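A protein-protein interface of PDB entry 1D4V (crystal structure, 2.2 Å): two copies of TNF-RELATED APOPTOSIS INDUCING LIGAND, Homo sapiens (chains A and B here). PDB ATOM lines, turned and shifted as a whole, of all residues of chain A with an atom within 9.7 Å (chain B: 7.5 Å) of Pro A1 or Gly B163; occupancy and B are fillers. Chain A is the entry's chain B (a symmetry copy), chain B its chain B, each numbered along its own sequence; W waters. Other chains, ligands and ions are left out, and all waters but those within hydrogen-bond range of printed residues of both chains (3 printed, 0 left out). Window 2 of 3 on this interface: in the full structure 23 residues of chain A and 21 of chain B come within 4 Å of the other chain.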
ATOM      1  N   PRO A   1     -21.258  15.264  -1.785  1.00  0.00           N
ATOM      2  CA  PRO A   1     -20.903  14.164  -0.850  1.00  0.00           C
ATOM      3  C   PRO A   1     -19.542  13.527  -1.162  1.00  0.00           C
ATOM      4  O   PRO A   1     -18.711  14.128  -1.848  1.00  0.00           O
ATOM      5  CB  PRO A   1     -22.028  13.142  -0.935  1.00  0.00           C
ATOM      6  CG  PRO A   1     -23.216  14.045  -1.301  1.00  0.00           C
ATOM      7  CD  PRO A   1     -22.629  15.072  -2.292  1.00  0.00           C
ATOM      8  N   GLN A   2     -19.331  12.311  -0.655  1.00  0.00           N
ATOM      9  CA  GLN A   2     -18.082  11.566  -0.833  1.00  0.00           C
ATOM     10  C   GLN A   2     -17.382  11.758  -2.183  1.00  0.00           C
ATOM     11  O   GLN A   2     -17.889  11.333  -3.217  1.00  0.00           O
ATOM     12  CB  GLN A   2     -18.341  10.078  -0.616  1.00  0.00           C
ATOM     13  CG  GLN A   2     -17.114   9.334  -0.157  1.00  0.00           C
ATOM     14  CD  GLN A   2     -16.590   9.884   1.152  1.00  0.00           C
ATOM     15  OE1 GLN A   2     -17.262   9.807   2.183  1.00  0.00           O
ATOM     16  NE2 GLN A   2     -15.387  10.457   1.119  1.00  0.00           N
ATOM     17  N   ARG A   3     -16.197  12.368  -2.159  1.00  0.00           N
ATOM     18  CA  ARG A   3     -15.445  12.642  -3.383  1.00  0.00           C
ATOM     19  C   ARG A   3     -14.599  11.483  -3.910  1.00  0.00           C
ATOM     20  O   ARG A   3     -13.805  10.890  -3.170  1.00  0.00           O
ATOM     21  CB  ARG A   3     -14.534  13.855  -3.180  1.00  0.00           C
ATOM     22  CG  ARG A   3     -15.219  15.090  -2.598  1.00  0.00           C
ATOM     23  CD  ARG A   3     -14.471  16.356  -3.026  1.00  0.00           C
ATOM     24  NE  ARG A   3     -14.142  17.285  -1.942  1.00  0.00           N
ATOM     25  CZ  ARG A   3     -13.364  17.001  -0.897  1.00  0.00           C
ATOM     26  NH1 ARG A   3     -12.819  15.797  -0.756  1.00  0.00           N
ATOM     27  NH2 ARG A   3     -13.110  17.942   0.004  1.00  0.00           N
ATOM     28  N   VAL A   4     -14.769  11.171  -5.196  1.00  0.00           N
ATOM     29  CA  VAL A   4     -14.012  10.097  -5.838  1.00  0.00           C
ATOM     30  C   VAL A   4     -13.066  10.672  -6.908  1.00  0.00           C
ATOM     31  O   VAL A   4     -13.479  10.958  -8.029  1.00  0.00           O
ATOM     32  CB  VAL A   4     -14.943   9.100  -6.509  1.00  0.00           C
ATOM     33  CG1 VAL A   4     -14.137   7.925  -7.038  1.00  0.00           C
ATOM     34  CG2 VAL A   4     -15.990   8.636  -5.522  1.00  0.00           C
ATOM     35  N   ALA A   5     -11.798  10.826  -6.550  1.00  0.00           N
ATOM     36  CA  ALA A   5     -10.808  11.386  -7.456  1.00  0.00           C
ATOM     37  C   ALA A   5      -9.392  11.157  -6.951  1.00  0.00           C
ATOM     38  O   ALA A   5      -9.185  10.801  -5.794  1.00  0.00           O
ATOM     39  CB  ALA A   5     -11.046  12.865  -7.611  1.00  0.00           C
ATOM     40  N   ALA A   6      -8.427  11.368  -7.838  1.00  0.00           N
ATOM     41  CA  ALA A   6      -7.019  11.208  -7.529  1.00  0.00           C
ATOM     42  C   ALA A   6      -6.153  12.002  -8.486  1.00  0.00           C
ATOM     43  O   ALA A   6      -6.530  12.218  -9.629  1.00  0.00           O
ATOM     44  CB  ALA A   6      -6.642   9.757  -7.637  1.00  0.00           C
ATOM     45  N   PHE A  45      -2.982  13.540  -4.212  1.00  0.00           N
ATOM     46  CA  PHE A  45      -3.922  12.983  -3.246  1.00  0.00           C
ATOM     47  C   PHE A  45      -4.675  11.821  -3.877  1.00  0.00           C
ATOM     48  O   PHE A  45      -4.669  11.662  -5.092  1.00  0.00           O
ATOM     49  CB  PHE A  45      -4.944  14.043  -2.806  1.00  0.00           C
ATOM     50  CG  PHE A  45      -5.912  14.428  -3.885  1.00  0.00           C
ATOM     51  CD1 PHE A  45      -5.512  15.279  -4.918  1.00  0.00           C
ATOM     52  CD2 PHE A  45      -7.186  13.855  -3.931  1.00  0.00           C
ATOM     53  CE1 PHE A  45      -6.361  15.553  -6.008  1.00  0.00           C
ATOM     54  CE2 PHE A  45      -8.048  14.115  -5.007  1.00  0.00           C
ATOM     55  CZ  PHE A  45      -7.623  14.972  -6.062  1.00  0.00           C
ATOM     56  N   SER A  47      -8.544  10.011  -3.199  1.00  0.00           N
ATOM     57  CA  SER A  47      -9.784  10.016  -2.460  1.00  0.00           C
ATOM     58  C   SER A  47     -10.674   8.945  -3.059  1.00  0.00           C
ATOM     59  O   SER A  47     -11.149   9.068  -4.186  1.00  0.00           O
ATOM     60  CB  SER A  47     -10.445  11.378  -2.559  1.00  0.00           C
ATOM     61  OG  SER A  47     -11.691  11.380  -1.893  1.00  0.00           O
ATOM     62  N   ASN A  48     -10.872   7.885  -2.285  1.00  0.00           N
ATOM     63  CA  ASN A  48     -11.677   6.747  -2.689  1.00  0.00           C
ATOM     64  C   ASN A  48     -11.143   6.024  -3.902  1.00  0.00           C
ATOM     65  O   ASN A  48     -11.888   5.602  -4.771  1.00  0.00           O
ATOM     66  CB  ASN A  48     -13.118   7.168  -2.898  1.00  0.00           C
ATOM     67  CG  ASN A  48     -13.821   7.453  -1.575  1.00  0.00           C
ATOM     68  OD1 ASN A  48     -13.816   6.616  -0.668  1.00  0.00           O
ATOM     69  ND2 ASN A  48     -14.427   8.622  -1.460  1.00  0.00           N
ATOM     70  N   GLU A  60     -15.206   2.547  -6.565  1.00  0.00           N
ATOM     71  CA  GLU A  60     -16.593   2.773  -6.960  1.00  0.00           C
ATOM     72  C   GLU A  60     -16.805   2.717  -8.473  1.00  0.00           C
ATOM     73  O   GLU A  60     -16.187   3.469  -9.222  1.00  0.00           O
ATOM     74  CB  GLU A  60     -17.067   4.128  -6.431  1.00  0.00           C
ATOM     75  CG  GLU A  60     -17.619   4.119  -5.004  1.00  0.00           C
ATOM     76  CD  GLU A  60     -18.218   5.470  -4.604  1.00  0.00           C
ATOM     77  OE1 GLU A  60     -19.046   6.014  -5.380  1.00  0.00           O
ATOM     78  OE2 GLU A  60     -17.865   5.984  -3.512  1.00  0.00           O
ATOM     79  N   ALA A 159      -7.640  11.006 -12.119  1.00  0.00           N
ATOM     80  CA  ALA A 159      -8.963  10.612 -12.583  1.00  0.00           C
ATOM     81  C   ALA A 159      -9.979  11.086 -11.586  1.00  0.00           C
ATOM     82  O   ALA A 159      -9.638  11.339 -10.442  1.00  0.00           O
ATOM     83  CB  ALA A 159      -9.061   9.086 -12.710  1.00  0.00           C
ATOM     84  N   PHE A 160     -11.226  11.230 -12.023  1.00  0.00           N
ATOM     85  CA  PHE A 160     -12.278  11.606 -11.090  1.00  0.00           C
ATOM     86  C   PHE A 160     -13.579  11.084 -11.642  1.00  0.00           C
ATOM     87  O   PHE A 160     -13.721  10.867 -12.848  1.00  0.00           O
ATOM     88  CB  PHE A 160     -12.349  13.117 -10.861  1.00  0.00           C
ATOM     89  CG  PHE A 160     -12.489  13.922 -12.125  1.00  0.00           C
ATOM     90  CD1 PHE A 160     -13.740  14.159 -12.672  1.00  0.00           C
ATOM     91  CD2 PHE A 160     -11.360  14.496 -12.737  1.00  0.00           C
ATOM     92  CE1 PHE A 160     -13.877  14.971 -13.813  1.00  0.00           C
ATOM     93  CE2 PHE A 160     -11.480  15.298 -13.857  1.00  0.00           C
ATOM     94  CZ  PHE A 160     -12.750  15.541 -14.402  1.00  0.00           C
ATOM     95  N   LEU A 161     -14.519  10.850 -10.737  1.00  0.00           N
ATOM     96  CA  LEU A 161     -15.824  10.329 -11.089  1.00  0.00           C
ATOM     97  C   LEU A 161     -16.628  11.348 -11.852  1.00  0.00           C
ATOM     98  O   LEU A 161     -16.838  12.456 -11.388  1.00  0.00           O
ATOM     99  CB  LEU A 161     -16.584   9.978  -9.832  1.00  0.00           C
ATOM    100  CG  LEU A 161     -17.011   8.547  -9.611  1.00  0.00           C
ATOM    101  CD1 LEU A 161     -18.066   8.568  -8.503  1.00  0.00           C
ATOM    102  CD2 LEU A 161     -17.586   7.959 -10.852  1.00  0.00           C
ATOM    103  N   VAL A 162     -17.100  10.969 -13.030  1.00  0.00           N
ATOM    104  CA  VAL A 162     -17.887  11.890 -13.804  1.00  0.00           C
ATOM    105  C   VAL A 162     -19.384  11.692 -13.613  1.00  0.00           C
ATOM    106  O   VAL A 162     -19.870  10.568 -13.459  1.00  0.00           O
ATOM    107  CB  VAL A 162     -17.515  11.792 -15.284  1.00  0.00           C
ATOM    108  CG1 VAL A 162     -18.670  12.205 -16.150  1.00  0.00           C
ATOM    109  CG2 VAL A 162     -16.355  12.700 -15.546  1.00  0.00           C
ATOM    110  N   GLY A 163     -20.100  12.814 -13.601  1.00  0.00           N
ATOM    111  CA  GLY A 163     -21.543  12.793 -13.435  1.00  0.00           C
ATOM    112  C   GLY A 163     -22.057  12.262 -12.109  1.00  0.00           C
ATOM    113  O   GLY A 163     -21.247  11.785 -11.278  1.00  0.00           O
ATOM    114  OXT GLY A 163     -23.290  12.322 -11.905  1.00  0.00           O
ATOM    115  N   PHE B  63     -11.497  20.242  -4.412  1.00  0.00           N
ATOM    116  CA  PHE B  63     -10.646  19.679  -5.439  1.00  0.00           C
ATOM    117  C   PHE B  63     -11.089  20.325  -6.740  1.00  0.00           C
ATOM    118  O   PHE B  63     -12.287  20.324  -7.083  1.00  0.00           O
ATOM    119  CB  PHE B  63     -10.848  18.173  -5.524  1.00  0.00           C
ATOM    120  CG  PHE B  63     -10.414  17.440  -4.297  1.00  0.00           C
ATOM    121  CD1 PHE B  63     -11.140  16.346  -3.839  1.00  0.00           C
ATOM    122  CD2 PHE B  63      -9.279  17.839  -3.595  1.00  0.00           C
ATOM    123  CE1 PHE B  63     -10.738  15.663  -2.693  1.00  0.00           C
ATOM    124  CE2 PHE B  63      -8.870  17.169  -2.456  1.00  0.00           C
ATOM    125  CZ  PHE B  63      -9.598  16.081  -1.999  1.00  0.00           C
ATOM    126  N   TYR B  64     -10.140  20.922  -7.447  1.00  0.00           N
ATOM    127  CA  TYR B  64     -10.471  21.549  -8.720  1.00  0.00           C
ATOM    128  C   TYR B  64      -9.664  20.993  -9.880  1.00  0.00           C
ATOM    129  O   TYR B  64      -8.450  20.810  -9.757  1.00  0.00           O
ATOM    130  CB  TYR B  64     -10.215  23.054  -8.677  1.00  0.00           C
ATOM    131  CG  TYR B  64     -11.214  23.867  -7.879  1.00  0.00           C
ATOM    132  CD1 TYR B  64     -11.220  23.832  -6.487  1.00  0.00           C
ATOM    133  CD2 TYR B  64     -12.144  24.677  -8.526  1.00  0.00           C
ATOM    134  CE1 TYR B  64     -12.132  24.587  -5.750  1.00  0.00           C
ATOM    135  CE2 TYR B  64     -13.065  25.443  -7.803  1.00  0.00           C
ATOM    136  CZ  TYR B  64     -13.056  25.395  -6.421  1.00  0.00           C
ATOM    137  OH  TYR B  64     -13.966  26.156  -5.716  1.00  0.00           O
ATOM    138  N   ILE B 129      -5.931  17.900 -11.340  1.00  0.00           N
ATOM    139  CA  ILE B 129      -6.666  18.261 -10.133  1.00  0.00           C
ATOM    140  C   ILE B 129      -5.829  18.634  -8.926  1.00  0.00           C
ATOM    141  O   ILE B 129      -4.890  17.938  -8.572  1.00  0.00           O
ATOM    142  CB  ILE B 129      -7.608  17.152  -9.696  1.00  0.00           C
ATOM    143  CG1 ILE B 129      -8.440  16.658 -10.878  1.00  0.00           C
ATOM    144  CG2 ILE B 129      -8.535  17.682  -8.629  1.00  0.00           C
ATOM    145  CD1 ILE B 129      -9.061  15.284 -10.599  1.00  0.00           C
ATOM    146  N   PHE B 160     -13.082  23.818 -12.552  1.00  0.00           N
ATOM    147  CA  PHE B 160     -14.400  23.486 -12.028  1.00  0.00           C
ATOM    148  C   PHE B 160     -14.199  22.573 -10.847  1.00  0.00           C
ATOM    149  O   PHE B 160     -13.179  21.889 -10.733  1.00  0.00           O
ATOM    150  CB  PHE B 160     -15.302  22.833 -13.076  1.00  0.00           C
ATOM    151  CG  PHE B 160     -14.701  21.617 -13.729  1.00  0.00           C
ATOM    152  CD1 PHE B 160     -14.834  20.369 -13.145  1.00  0.00           C
ATOM    153  CD2 PHE B 160     -14.049  21.721 -14.972  1.00  0.00           C
ATOM    154  CE1 PHE B 160     -14.335  19.222 -13.790  1.00  0.00           C
ATOM    155  CE2 PHE B 160     -13.557  20.603 -15.620  1.00  0.00           C
ATOM    156  CZ  PHE B 160     -13.701  19.339 -15.026  1.00  0.00           C
ATOM    157  N   LEU B 161     -15.172  22.597  -9.948  1.00  0.00           N
ATOM    158  CA  LEU B 161     -15.136  21.795  -8.742  1.00  0.00           C
ATOM    159  C   LEU B 161     -15.285  20.330  -9.057  1.00  0.00           C
ATOM    160  O   LEU B 161     -16.245  19.920  -9.687  1.00  0.00           O
ATOM    161  CB  LEU B 161     -16.273  22.197  -7.833  1.00  0.00           C
ATOM    162  CG  LEU B 161     -15.956  22.745  -6.462  1.00  0.00           C
ATOM    163  CD1 LEU B 161     -17.253  22.688  -5.653  1.00  0.00           C
ATOM    164  CD2 LEU B 161     -14.898  21.941  -5.791  1.00  0.00           C
ATOM    165  N   VAL B 162     -14.336  19.527  -8.602  1.00  0.00           N
ATOM    166  CA  VAL B 162     -14.425  18.114  -8.857  1.00  0.00           C
ATOM    167  C   VAL B 162     -15.046  17.345  -7.701  1.00  0.00           C
ATOM    168  O   VAL B 162     -14.837  17.666  -6.528  1.00  0.00           O
ATOM    169  CB  VAL B 162     -13.047  17.550  -9.203  1.00  0.00           C
ATOM    170  CG1 VAL B 162     -12.967  16.093  -8.849  1.00  0.00           C
ATOM    171  CG2 VAL B 162     -12.819  17.712 -10.672  1.00  0.00           C
ATOM    172  N   GLY B 163     -15.836  16.335  -8.060  1.00  0.00           N
ATOM    173  CA  GLY B 163     -16.496  15.499  -7.073  1.00  0.00           C
ATOM    174  C   GLY B 163     -17.517  16.190  -6.186  1.00  0.00           C
ATOM    175  O   GLY B 163     -17.667  17.433  -6.268  1.00  0.00           O
ATOM    176  OXT GLY B 163     -18.168  15.473  -5.394  1.00  0.00           O
HETATM  177  O   HOH W   1     -15.832  13.824  -9.280  1.00  0.00           O
HETATM  178  O   HOH W   2     -16.581  12.770  -6.717  1.00  0.00           O
HETATM  179  O   HOH W   3     -13.833  19.056  -4.141  1.00  0.00           O
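Water W3 lies within hydrogen-bond range of N of Phe B63 (2.6 Å), NE of Arg A3 (2.8 Å) and O of Val B162 (2.9 Å).
Water W1 lies within hydrogen-bond range of O of Leu A161 (2.7 Å) and N of Gly B163 (2.8 Å).
Water W2 bridges N of Val A4 (2.9 Å) and OXT of Gly B163 (3.4 Å).
Among the printed residues, pairs that only touch across the chains: Pro A1 with Gly B163, Arg A3 with Phe B63, Arg A3 with Val B162, Ala A5 with Val B162, Phe A45 with Phe B63, Phe A45 with Ile B129, Ala A159 with Ile B129, Phe A160 with Ile B129, Phe A160 with Phe B160 and Phe A160 with Val B162.
Pro A1 touches just one residue of chain B: Gly B163.
Gln A2 touches none of the printed residues of chain B.
Of the printed residues of chain B, Ala A159 touches Ile B129.
Leu A161 touches none of the printed residues of chain B.
Of the printed residues of chain A, Phe B63 touches Arg A3 and Phe A45.
Printed residues of chain A within 4 Å of Ile B129: Phe A45, Ala A159 and Phe A160.
Of the printed residues of chain A, Phe B160 touches Phe A160.
Val B162 touches three residues of chain A.
Of chain A, only Pro A1 (3.8 Å) comes within 4 Å of Gly B163.
Hydrophobic or aromatic side chains of chain A that line the printed part of chain B: Ala A5, Phe A45 and Phe A160.
Of the 7 printed residues of chain B, 5 touch a printed residue of chain A.
Printed residues of chain B that touch a printed residue of chain A: Phe B63, Ile B129, Phe B160, Val B162 and Gly B163.
Among the printed residues, 10 pairs touch across the chains.
Among the printed residues, no Asp or Glu carboxylate lies within 4 Å of a Lys or Arg side-chain nitrogen of the other chain.
Phe B160 touches its own counterpart, Phe A160.
Phe A160 touches Val B162, but with the chains exchanged Val A162 does not touch Phe B160 (7.0 Å).
The backbone carbonyl oxygen (O) of Phe B63 is in hydrogen-bond range of the backbone NH (N) of Val B162 (2.7 Å).
The backbone carbonyl oxygen (O) of Arg A3 is in hydrogen-bond range of the side-chain hydroxyl (OG) of Ser A47 (2.5 Å).
The backbone carbonyl oxygen (O) of Arg A3 is in hydrogen-bond range of the side-chain amide nitrogen (ND2) of Asn A48, 2.9 Å away.
N of Ser A47 sits at hydrogen-bond distance from O of Ala A5 (2.8 Å).
The backbone NH (N) of Ala A6 is in hydrogen-bond range of the backbone carbonyl oxygen (O) of Ala A159, at 2.9 Å.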
